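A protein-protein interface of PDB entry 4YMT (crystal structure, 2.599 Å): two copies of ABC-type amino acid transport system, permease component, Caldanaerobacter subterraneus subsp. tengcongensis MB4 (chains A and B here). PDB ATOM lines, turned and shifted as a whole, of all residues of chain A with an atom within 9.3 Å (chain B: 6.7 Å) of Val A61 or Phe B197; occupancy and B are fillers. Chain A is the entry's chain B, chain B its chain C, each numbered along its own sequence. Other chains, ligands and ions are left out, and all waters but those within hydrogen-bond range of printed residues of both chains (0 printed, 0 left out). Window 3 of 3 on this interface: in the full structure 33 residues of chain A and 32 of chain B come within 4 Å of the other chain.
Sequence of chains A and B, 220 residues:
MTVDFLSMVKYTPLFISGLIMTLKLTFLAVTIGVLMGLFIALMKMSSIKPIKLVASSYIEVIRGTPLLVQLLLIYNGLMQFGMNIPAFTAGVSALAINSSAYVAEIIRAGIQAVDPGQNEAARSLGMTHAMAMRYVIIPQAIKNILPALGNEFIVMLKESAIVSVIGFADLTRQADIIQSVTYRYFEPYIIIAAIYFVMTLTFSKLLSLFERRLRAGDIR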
ATOM      1  N   LEU A  53     -30.933  -1.173  21.484  1.00  0.00           N
ATOM      2  CA  LEU A  53     -29.792  -0.301  21.184  1.00  0.00           C
ATOM      3  C   LEU A  53     -29.920   0.365  19.810  1.00  0.00           C
ATOM      4  O   LEU A  53     -29.679   1.570  19.674  1.00  0.00           O
ATOM      5  CB  LEU A  53     -28.474  -1.082  21.245  1.00  0.00           C
ATOM      6  CG  LEU A  53     -27.264  -0.349  20.639  1.00  0.00           C
ATOM      7  CD1 LEU A  53     -26.880   0.890  21.465  1.00  0.00           C
ATOM      8  CD2 LEU A  53     -26.059  -1.274  20.422  1.00  0.00           C
ATOM      9  N   VAL A  54     -30.278  -0.420  18.794  1.00  0.00           N
ATOM     10  CA  VAL A  54     -30.391   0.112  17.435  1.00  0.00           C
ATOM     11  C   VAL A  54     -31.529   1.136  17.352  1.00  0.00           C
ATOM     12  O   VAL A  54     -31.332   2.209  16.782  1.00  0.00           O
ATOM     13  CB  VAL A  54     -30.541  -1.021  16.348  1.00  0.00           C
ATOM     14  CG1 VAL A  54     -31.986  -1.462  16.127  1.00  0.00           C
ATOM     15  CG2 VAL A  54     -29.924  -0.573  15.028  1.00  0.00           C
ATOM     16  N   ALA A  55     -32.708   0.817  17.901  1.00  0.00           N
ATOM     17  CA  ALA A  55     -33.832   1.756  17.859  1.00  0.00           C
ATOM     18  C   ALA A  55     -33.464   3.051  18.581  1.00  0.00           C
ATOM     19  O   ALA A  55     -33.770   4.165  18.113  1.00  0.00           O
ATOM     20  CB  ALA A  55     -35.075   1.141  18.464  1.00  0.00           C
ATOM     21  N   SER A  56     -32.813   2.896  19.729  1.00  0.00           N
ATOM     22  CA  SER A  56     -32.390   4.043  20.516  1.00  0.00           C
ATOM     23  C   SER A  56     -31.426   4.926  19.694  1.00  0.00           C
ATOM     24  O   SER A  56     -31.606   6.146  19.610  1.00  0.00           O
ATOM     25  CB  SER A  56     -31.753   3.570  21.831  1.00  0.00           C
ATOM     26  OG  SER A  56     -31.277   4.652  22.612  1.00  0.00           O
ATOM     27  N   SER A  57     -30.425   4.304  19.070  1.00  0.00           N
ATOM     28  CA  SER A  57     -29.430   5.044  18.280  1.00  0.00           C
ATOM     29  C   SER A  57     -30.034   5.728  17.040  1.00  0.00           C
ATOM     30  O   SER A  57     -29.725   6.886  16.754  1.00  0.00           O
ATOM     31  CB  SER A  57     -28.288   4.116  17.870  1.00  0.00           C
ATOM     32  OG  SER A  57     -27.642   3.592  19.015  1.00  0.00           O
ATOM     33  N   TYR A  58     -30.869   4.997  16.301  1.00  0.00           N
ATOM     34  CA  TYR A  58     -31.655   5.561  15.211  1.00  0.00           C
ATOM     35  C   TYR A  58     -32.338   6.844  15.651  1.00  0.00           C
ATOM     36  O   TYR A  58     -32.093   7.915  15.086  1.00  0.00           O
ATOM     37  CB  TYR A  58     -32.695   4.551  14.742  1.00  0.00           C
ATOM     38  CG  TYR A  58     -33.608   5.015  13.620  1.00  0.00           C
ATOM     39  CD1 TYR A  58     -33.456   4.528  12.316  1.00  0.00           C
ATOM     40  CD2 TYR A  58     -34.647   5.907  13.866  1.00  0.00           C
ATOM     41  CE1 TYR A  58     -34.307   4.930  11.299  1.00  0.00           C
ATOM     42  CE2 TYR A  58     -35.492   6.319  12.854  1.00  0.00           C
ATOM     43  CZ  TYR A  58     -35.322   5.829  11.575  1.00  0.00           C
ATOM     44  OH  TYR A  58     -36.180   6.246  10.590  1.00  0.00           O
ATOM     45  N   ILE A  59     -33.190   6.717  16.671  1.00  0.00           N
ATOM     46  CA  ILE A  59     -33.988   7.837  17.182  1.00  0.00           C
ATOM     47  C   ILE A  59     -33.115   9.022  17.593  1.00  0.00           C
ATOM     48  O   ILE A  59     -33.310  10.153  17.133  1.00  0.00           O
ATOM     49  CB  ILE A  59     -34.848   7.378  18.374  1.00  0.00           C
ATOM     50  CG1 ILE A  59     -35.927   6.408  17.889  1.00  0.00           C
ATOM     51  CG2 ILE A  59     -35.467   8.562  19.077  1.00  0.00           C
ATOM     52  CD1 ILE A  59     -36.673   5.719  18.998  1.00  0.00           C
ATOM     53  N   GLU A  60     -32.133   8.735  18.437  1.00  0.00           N
ATOM     54  CA  GLU A  60     -31.198   9.738  18.919  1.00  0.00           C
ATOM     55  C   GLU A  60     -30.483  10.483  17.792  1.00  0.00           C
ATOM     56  O   GLU A  60     -30.316  11.705  17.856  1.00  0.00           O
ATOM     57  CB  GLU A  60     -30.168   9.078  19.840  1.00  0.00           C
ATOM     58  CG  GLU A  60     -29.585  10.005  20.889  1.00  0.00           C
ATOM     59  CD  GLU A  60     -28.773   9.263  21.930  1.00  0.00           C
ATOM     60  OE1 GLU A  60     -28.866   8.014  21.968  1.00  0.00           O
ATOM     61  OE2 GLU A  60     -28.027   9.927  22.689  1.00  0.00           O
ATOM     62  N   VAL A  61     -30.089   9.757  16.748  1.00  0.00           N
ATOM     63  CA  VAL A  61     -29.332  10.362  15.648  1.00  0.00           C
ATOM     64  C   VAL A  61     -30.246  11.202  14.766  1.00  0.00           C
ATOM     65  O   VAL A  61     -29.969  12.375  14.568  1.00  0.00           O
ATOM     66  CB  VAL A  61     -28.603   9.299  14.780  1.00  0.00           C
ATOM     67  CG1 VAL A  61     -28.068   9.932  13.528  1.00  0.00           C
ATOM     68  CG2 VAL A  61     -27.462   8.663  15.558  1.00  0.00           C
ATOM     69  N   ILE A  62     -31.333  10.610  14.265  1.00  0.00           N
ATOM     70  CA  ILE A  62     -32.299  11.334  13.435  1.00  0.00           C
ATOM     71  C   ILE A  62     -32.817  12.612  14.125  1.00  0.00           C
ATOM     72  O   ILE A  62     -33.010  13.654  13.486  1.00  0.00           O
ATOM     73  CB  ILE A  62     -33.485  10.432  13.058  1.00  0.00           C
ATOM     74  CG1 ILE A  62     -33.005   9.167  12.348  1.00  0.00           C
ATOM     75  CG2 ILE A  62     -34.444  11.163  12.153  1.00  0.00           C
ATOM     76  CD1 ILE A  62     -32.361   9.439  11.001  1.00  0.00           C
ATOM     77  N   ARG A  63     -33.024  12.547  15.436  1.00  0.00           N
ATOM     78  CA  ARG A  63     -33.521  13.716  16.150  1.00  0.00           C
ATOM     79  C   ARG A  63     -32.379  14.673  16.500  1.00  0.00           C
ATOM     80  O   ARG A  63     -32.582  15.899  16.582  1.00  0.00           O
ATOM     81  CB  ARG A  63     -34.279  13.302  17.431  1.00  0.00           C
ATOM     82  CG  ARG A  63     -35.582  12.522  17.204  1.00  0.00           C
ATOM     83  CD  ARG A  63     -36.240  12.145  18.529  1.00  0.00           C
ATOM     84  NE  ARG A  63     -36.867  13.309  19.142  1.00  0.00           N
ATOM     85  CZ  ARG A  63     -36.602  13.734  20.370  1.00  0.00           C
ATOM     86  NH1 ARG A  63     -35.712  13.084  21.118  1.00  0.00           N
ATOM     87  NH2 ARG A  63     -37.213  14.818  20.840  1.00  0.00           N
ATOM     88  N   GLY A  64     -31.187  14.118  16.715  1.00  0.00           N
ATOM     89  CA  GLY A  64     -30.049  14.912  17.147  1.00  0.00           C
ATOM     90  C   GLY A  64     -29.298  15.571  16.004  1.00  0.00           C
ATOM     91  O   GLY A  64     -28.231  16.167  16.208  1.00  0.00           O
ATOM     92  N   THR A  65     -29.876  15.488  14.804  1.00  0.00           N
ATOM     93  CA  THR A  65     -29.211  15.918  13.577  1.00  0.00           C
ATOM     94  C   THR A  65     -30.202  16.631  12.619  1.00  0.00           C
ATOM     95  O   THR A  65     -31.390  16.283  12.593  1.00  0.00           O
ATOM     96  CB  THR A  65     -28.537  14.671  12.920  1.00  0.00           C
ATOM     97  OG1 THR A  65     -27.325  15.054  12.271  1.00  0.00           O
ATOM     98  CG2 THR A  65     -29.467  13.926  11.967  1.00  0.00           C
ATOM     99  N   PRO A  66     -29.729  17.641  11.842  1.00  0.00           N
ATOM    100  CA  PRO A  66     -30.644  18.481  11.040  1.00  0.00           C
ATOM    101  C   PRO A  66     -31.408  17.756   9.927  1.00  0.00           C
ATOM    102  O   PRO A  66     -30.866  16.842   9.293  1.00  0.00           O
ATOM    103  CB  PRO A  66     -29.708  19.539  10.428  1.00  0.00           C
ATOM    104  CG  PRO A  66     -28.518  19.574  11.327  1.00  0.00           C
ATOM    105  CD  PRO A  66     -28.341  18.142  11.773  1.00  0.00           C
ATOM    106  N   LEU A  67     -32.645  18.183   9.678  1.00  0.00           N
ATOM    107  CA  LEU A  67     -33.449  17.628   8.588  1.00  0.00           C
ATOM    108  C   LEU A  67     -32.767  17.873   7.230  1.00  0.00           C
ATOM    109  O   LEU A  67     -32.771  16.999   6.367  1.00  0.00           O
ATOM    110  CB  LEU A  67     -34.849  18.247   8.582  1.00  0.00           C
ATOM    111  CG  LEU A  67     -36.055  17.469   8.027  1.00  0.00           C
ATOM    112  CD1 LEU A  67     -36.923  18.381   7.174  1.00  0.00           C
ATOM    113  CD2 LEU A  67     -35.705  16.180   7.287  1.00  0.00           C
ATOM    114  N   VAL A  69     -29.546  18.205   6.355  1.00  0.00           N
ATOM    115  CA  VAL A  69     -28.454  17.269   6.134  1.00  0.00           C
ATOM    116  C   VAL A  69     -28.988  15.861   5.807  1.00  0.00           C
ATOM    117  O   VAL A  69     -28.367  15.133   5.056  1.00  0.00           O
ATOM    118  CB  VAL A  69     -27.500  17.270   7.338  1.00  0.00           C
ATOM    119  CG1 VAL A  69     -26.334  16.340   7.128  1.00  0.00           C
ATOM    120  CG2 VAL A  69     -26.985  18.693   7.577  1.00  0.00           C
ATOM    121  N   GLN A  70     -30.156  15.490   6.327  1.00  0.00           N
ATOM    122  CA  GLN A  70     -30.755  14.189   5.987  1.00  0.00           C
ATOM    123  C   GLN A  70     -31.270  14.169   4.544  1.00  0.00           C
ATOM    124  O   GLN A  70     -31.069  13.187   3.794  1.00  0.00           O
ATOM    125  CB  GLN A  70     -31.884  13.853   6.964  1.00  0.00           C
ATOM    126  CG  GLN A  70     -31.380  13.630   8.381  1.00  0.00           C
ATOM    127  CD  GLN A  70     -32.466  13.637   9.463  1.00  0.00           C
ATOM    128  OE1 GLN A  70     -32.169  13.929  10.612  1.00  0.00           O
ATOM    129  NE2 GLN A  70     -33.709  13.313   9.104  1.00  0.00           N
ATOM    130  N   LEU A  73     -28.153  14.311   2.272  1.00  0.00           N
ATOM    131  CA  LEU A  73     -27.473  13.019   2.350  1.00  0.00           C
ATOM    132  C   LEU A  73     -28.179  11.970   1.490  1.00  0.00           C
ATOM    133  O   LEU A  73     -27.521  11.139   0.853  1.00  0.00           O
ATOM    134  CB  LEU A  73     -27.382  12.536   3.797  1.00  0.00           C
ATOM    135  CG  LEU A  73     -26.671  11.217   4.093  1.00  0.00           C
ATOM    136  CD1 LEU A  73     -25.297  11.181   3.457  1.00  0.00           C
ATOM    137  CD2 LEU A  73     -26.558  11.056   5.602  1.00  0.00           C
ATOM    138  N   ILE A  97     -38.402   9.572   7.371  1.00  0.00           N
ATOM    139  CA  ILE A  97     -37.376   9.040   8.257  1.00  0.00           C
ATOM    140  C   ILE A  97     -37.180  10.008   9.422  1.00  0.00           C
ATOM    141  O   ILE A  97     -36.994   9.588  10.567  1.00  0.00           O
ATOM    142  CB  ILE A  97     -36.048   8.800   7.513  1.00  0.00           C
ATOM    143  CG1 ILE A  97     -36.122   7.521   6.680  1.00  0.00           C
ATOM    144  CG2 ILE A  97     -34.879   8.709   8.470  1.00  0.00           C
ATOM    145  CD1 ILE A  97     -34.937   7.361   5.739  1.00  0.00           C
ATOM    146  N   ASN A  98     -37.239  11.306   9.143  1.00  0.00           N
ATOM    147  CA  ASN A  98     -37.175  12.286  10.220  1.00  0.00           C
ATOM    148  C   ASN A  98     -38.387  12.166  11.165  1.00  0.00           C
ATOM    149  O   ASN A  98     -38.238  12.159  12.385  1.00  0.00           O
ATOM    150  CB  ASN A  98     -37.072  13.702   9.652  1.00  0.00           C
ATOM    151  CG  ASN A  98     -36.881  14.761  10.737  1.00  0.00           C
ATOM    152  OD1 ASN A  98     -37.804  15.517  11.039  1.00  0.00           O
ATOM    153  ND2 ASN A  98     -35.690  14.821  11.327  1.00  0.00           N
ATOM    154  N   ALA A 101     -38.631   9.105  13.809  1.00  0.00           N
ATOM    155  CA  ALA A 101     -37.890   9.177  15.059  1.00  0.00           C
ATOM    156  C   ALA A 101     -38.652  10.019  16.086  1.00  0.00           C
ATOM    157  O   ALA A 101     -38.706   9.686  17.280  1.00  0.00           O
ATOM    158  CB  ALA A 101     -36.503   9.749  14.825  1.00  0.00           C
ATOM    159  N   TYR A 102     -39.226  11.124  15.625  1.00  0.00           N
ATOM    160  CA  TYR A 102     -39.989  11.981  16.510  1.00  0.00           C
ATOM    161  C   TYR A 102     -41.284  11.280  16.958  1.00  0.00           C
ATOM    162  O   TYR A 102     -41.711  11.427  18.109  1.00  0.00           O
ATOM    163  CB  TYR A 102     -40.284  13.326  15.826  1.00  0.00           C
ATOM    164  CG  TYR A 102     -39.076  14.248  15.754  1.00  0.00           C
ATOM    165  CD1 TYR A 102     -38.876  15.235  16.707  1.00  0.00           C
ATOM    166  CD2 TYR A 102     -38.122  14.117  14.739  1.00  0.00           C
ATOM    167  CE1 TYR A 102     -37.772  16.076  16.651  1.00  0.00           C
ATOM    168  CE2 TYR A 102     -37.011  14.953  14.671  1.00  0.00           C
ATOM    169  CZ  TYR A 102     -36.839  15.934  15.629  1.00  0.00           C
ATOM    170  OH  TYR A 102     -35.737  16.778  15.576  1.00  0.00           O
ATOM    171  N   ILE B 192     -20.526  15.637   8.502  1.00  0.00           N
ATOM    172  CA  ILE B 192     -21.234  16.814   8.991  1.00  0.00           C
ATOM    173  C   ILE B 192     -22.324  16.444  10.018  1.00  0.00           C
ATOM    174  O   ILE B 192     -22.461  17.102  11.062  1.00  0.00           O
ATOM    175  CB  ILE B 192     -21.840  17.607   7.822  1.00  0.00           C
ATOM    176  CG1 ILE B 192     -20.759  18.466   7.163  1.00  0.00           C
ATOM    177  CG2 ILE B 192     -22.954  18.527   8.298  1.00  0.00           C
ATOM    178  CD1 ILE B 192     -21.196  19.071   5.856  1.00  0.00           C
ATOM    179  N   ALA B 193     -23.105  15.409   9.699  1.00  0.00           N
ATOM    180  CA  ALA B 193     -24.135  14.900  10.598  1.00  0.00           C
ATOM    181  C   ALA B 193     -23.521  14.423  11.914  1.00  0.00           C
ATOM    182  O   ALA B 193     -24.093  14.620  12.974  1.00  0.00           O
ATOM    183  CB  ALA B 193     -24.922  13.780   9.940  1.00  0.00           C
ATOM    184  N   ALA B 194     -22.354  13.802  11.842  1.00  0.00           N
ATOM    185  CA  ALA B 194     -21.667  13.359  13.037  1.00  0.00           C
ATOM    186  C   ALA B 194     -21.274  14.565  13.883  1.00  0.00           C
ATOM    187  O   ALA B 194     -21.374  14.520  15.113  1.00  0.00           O
ATOM    188  CB  ALA B 194     -20.450  12.523  12.684  1.00  0.00           C
ATOM    189  N   ILE B 195     -20.821  15.637  13.238  1.00  0.00           N
ATOM    190  CA  ILE B 195     -20.467  16.850  13.981  1.00  0.00           C
ATOM    191  C   ILE B 195     -21.695  17.502  14.658  1.00  0.00           C
ATOM    192  O   ILE B 195     -21.634  17.898  15.839  1.00  0.00           O
ATOM    193  CB  ILE B 195     -19.798  17.907  13.083  1.00  0.00           C
ATOM    194  CG1 ILE B 195     -18.566  17.327  12.382  1.00  0.00           C
ATOM    195  CG2 ILE B 195     -19.439  19.136  13.907  1.00  0.00           C
ATOM    196  CD1 ILE B 195     -17.533  16.784  13.337  1.00  0.00           C
ATOM    197  N   TYR B 196     -22.808  17.588  13.923  1.00  0.00           N
ATOM    198  CA  TYR B 196     -24.046  18.149  14.469  1.00  0.00           C
ATOM    199  C   TYR B 196     -24.502  17.311  15.672  1.00  0.00           C
ATOM    200  O   TYR B 196     -24.839  17.844  16.729  1.00  0.00           O
ATOM    201  CB  TYR B 196     -25.156  18.205  13.406  1.00  0.00           C
ATOM    202  CG  TYR B 196     -25.133  19.438  12.524  1.00  0.00           C
ATOM    203  CD1 TYR B 196     -25.402  20.686  13.046  1.00  0.00           C
ATOM    204  CD2 TYR B 196     -24.863  19.344  11.157  1.00  0.00           C
ATOM    205  CE1 TYR B 196     -25.389  21.821  12.251  1.00  0.00           C
ATOM    206  CE2 TYR B 196     -24.850  20.478  10.347  1.00  0.00           C
ATOM    207  CZ  TYR B 196     -25.109  21.717  10.900  1.00  0.00           C
ATOM    208  OH  TYR B 196     -25.099  22.862  10.117  1.00  0.00           O
ATOM    209  N   PHE B 197     -24.490  15.998  15.495  1.00  0.00           N
ATOM    210  CA  PHE B 197     -24.850  15.052  16.542  1.00  0.00           C
ATOM    211  C   PHE B 197     -24.024  15.250  17.812  1.00  0.00           C
ATOM    212  O   PHE B 197     -24.589  15.442  18.902  1.00  0.00           O
ATOM    213  CB  PHE B 197     -24.667  13.637  16.015  1.00  0.00           C
ATOM    214  CG  PHE B 197     -25.167  12.565  16.928  1.00  0.00           C
ATOM    215  CD1 PHE B 197     -26.527  12.362  17.112  1.00  0.00           C
ATOM    216  CD2 PHE B 197     -24.274  11.718  17.568  1.00  0.00           C
ATOM    217  CE1 PHE B 197     -26.989  11.343  17.942  1.00  0.00           C
ATOM    218  CE2 PHE B 197     -24.729  10.704  18.390  1.00  0.00           C
ATOM    219  CZ  PHE B 197     -26.090  10.517  18.577  1.00  0.00           C
ATOM    220  N   VAL B 198     -22.696  15.240  17.666  1.00  0.00           N
ATOM    221  CA  VAL B 198     -21.822  15.411  18.822  1.00  0.00           C
ATOM    222  C   VAL B 198     -22.104  16.750  19.505  1.00  0.00           C
ATOM    223  O   VAL B 198     -22.125  16.824  20.739  1.00  0.00           O
ATOM    224  CB  VAL B 198     -20.332  15.293  18.446  1.00  0.00           C
ATOM    225  CG1 VAL B 198     -19.459  15.960  19.486  1.00  0.00           C
ATOM    226  CG2 VAL B 198     -19.952  13.836  18.331  1.00  0.00           C
ATOM    227  N   MET B 199     -22.351  17.797  18.716  1.00  0.00           N
ATOM    228  CA  MET B 199     -22.723  19.091  19.295  1.00  0.00           C
ATOM    229  C   MET B 199     -24.013  18.990  20.139  1.00  0.00           C
ATOM    230  O   MET B 199     -24.103  19.540  21.252  1.00  0.00           O
ATOM    231  CB  MET B 199     -22.901  20.136  18.200  1.00  0.00           C
ATOM    232  CG  MET B 199     -21.782  21.140  18.123  1.00  0.00           C
ATOM    233  SD  MET B 199     -22.287  22.549  17.113  1.00  0.00           S
ATOM    234  CE  MET B 199     -22.972  21.693  15.680  1.00  0.00           C
ATOM    235  N   THR B 200     -25.002  18.291  19.585  1.00  0.00           N
ATOM    236  CA  THR B 200     -26.280  18.088  20.239  1.00  0.00           C
ATOM    237  C   THR B 200     -26.110  17.353  21.567  1.00  0.00           C
ATOM    238  O   THR B 200     -26.611  17.800  22.585  1.00  0.00           O
ATOM    239  CB  THR B 200     -27.248  17.312  19.332  1.00  0.00           C
ATOM    240  OG1 THR B 200     -27.896  18.242  18.462  1.00  0.00           O
ATOM    241  CG2 THR B 200     -28.318  16.607  20.155  1.00  0.00           C
ATOM    242  N   LEU B 201     -25.394  16.233  21.550  1.00  0.00           N
ATOM    243  CA  LEU B 201     -25.153  15.475  22.768  1.00  0.00           C
ATOM    244  C   LEU B 201     -24.413  16.306  23.810  1.00  0.00           C
ATOM    245  O   LEU B 201     -24.844  16.392  24.961  1.00  0.00           O
ATOM    246  CB  LEU B 201     -24.361  14.201  22.464  1.00  0.00           C
ATOM    247  CG  LEU B 201     -25.122  13.104  21.720  1.00  0.00           C
ATOM    248  CD1 LEU B 201     -24.449  11.760  21.928  1.00  0.00           C
ATOM    249  CD2 LEU B 201     -26.578  13.048  22.158  1.00  0.00           C
ATOM    250  N   THR B 202     -23.314  16.923  23.394  1.00  0.00           N
ATOM    251  CA  THR B 202     -22.486  17.712  24.292  1.00  0.00           C
ATOM    252  C   THR B 202     -23.280  18.808  24.996  1.00  0.00           C
ATOM    253  O   THR B 202     -23.258  18.910  26.237  1.00  0.00           O
ATOM    254  CB  THR B 202     -21.314  18.336  23.527  1.00  0.00           C
ATOM    255  OG1 THR B 202     -20.544  17.286  22.928  1.00  0.00           O
ATOM    256  CG2 THR B 202     -20.425  19.167  24.454  1.00  0.00           C
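The side-chain hydroxyl (OG1) of Thr A65 lies within hydrogen-bond range of the backbone carbonyl oxygen (O) of Ala B193.
The side-chain hydroxyl of Thr B200 lies within hydrogen-bond range of the backbone carbonyl oxygen of Gly A64 (3.1 Å).
OE1 of Gln A70 sits close to O of Thr A65 (3.2 Å).
O of Pro A66 sits close to OE1 of Gln A70 (3.5 Å).
Among the printed residues, pairs that only touch across the chains: Glu A60 with Phe B197 (3.3 Å), Val A61 with Phe B197 (3.4 Å), Glu A60 with Leu B201 (3.5 Å), Pro A66 with Tyr B196 (3.5 Å), Gly A64 with Phe B197 (3.6 Å), Gly A64 with Tyr B196 (3.8 Å), Val A69 with Tyr B196 (3.9 Å) and Thr A65 with Tyr B196 (3.99 Å).
Of the printed residues of chain B, Glu A60 touches Phe B197 and Leu B201.
Val A61 touches just one residue of chain B: Phe B197.
Of the printed residues of chain B, Gly A64 touches Tyr B196, Phe B197 and Thr B200.
Of the printed residues of chain B, Thr A65 touches Ala B193 and Tyr B196.
Of chain A, only Glu A60 (3.3 Å), Val A61 (3.4 Å) and Gly A64 (3.6 Å) come within 4 Å of Phe B197.
No residue of chain A comes within 4 Å of Val B198.
Thr B200 touches one residue of chain A.
The nearest residue of chain B that does not touch Val A61 is Ala B193 (6.1 Å).
The nearest printed residue of chain A that does not touch Ala B193 is Val A69 (4.1 Å).
Of the 11 printed residues of chain B, 5 touch a printed residue of chain A.
Printed residues of chain B that touch a printed residue of chain A: Ala B193, Tyr B196, Phe B197, Thr B200 and Leu B201.
Along chain A the printed residues that touch a printed residue of chain B span positions 60 to 69.
Among the printed residues, no Asp or Glu carboxylate lies within 4 Å of a Lys or Arg side-chain nitrogen of the other chain.
No position is printed for both chains.
Of the 10 pairs that touch across the chains among the printed residues, none has its exchanged pair printed and touching as well.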
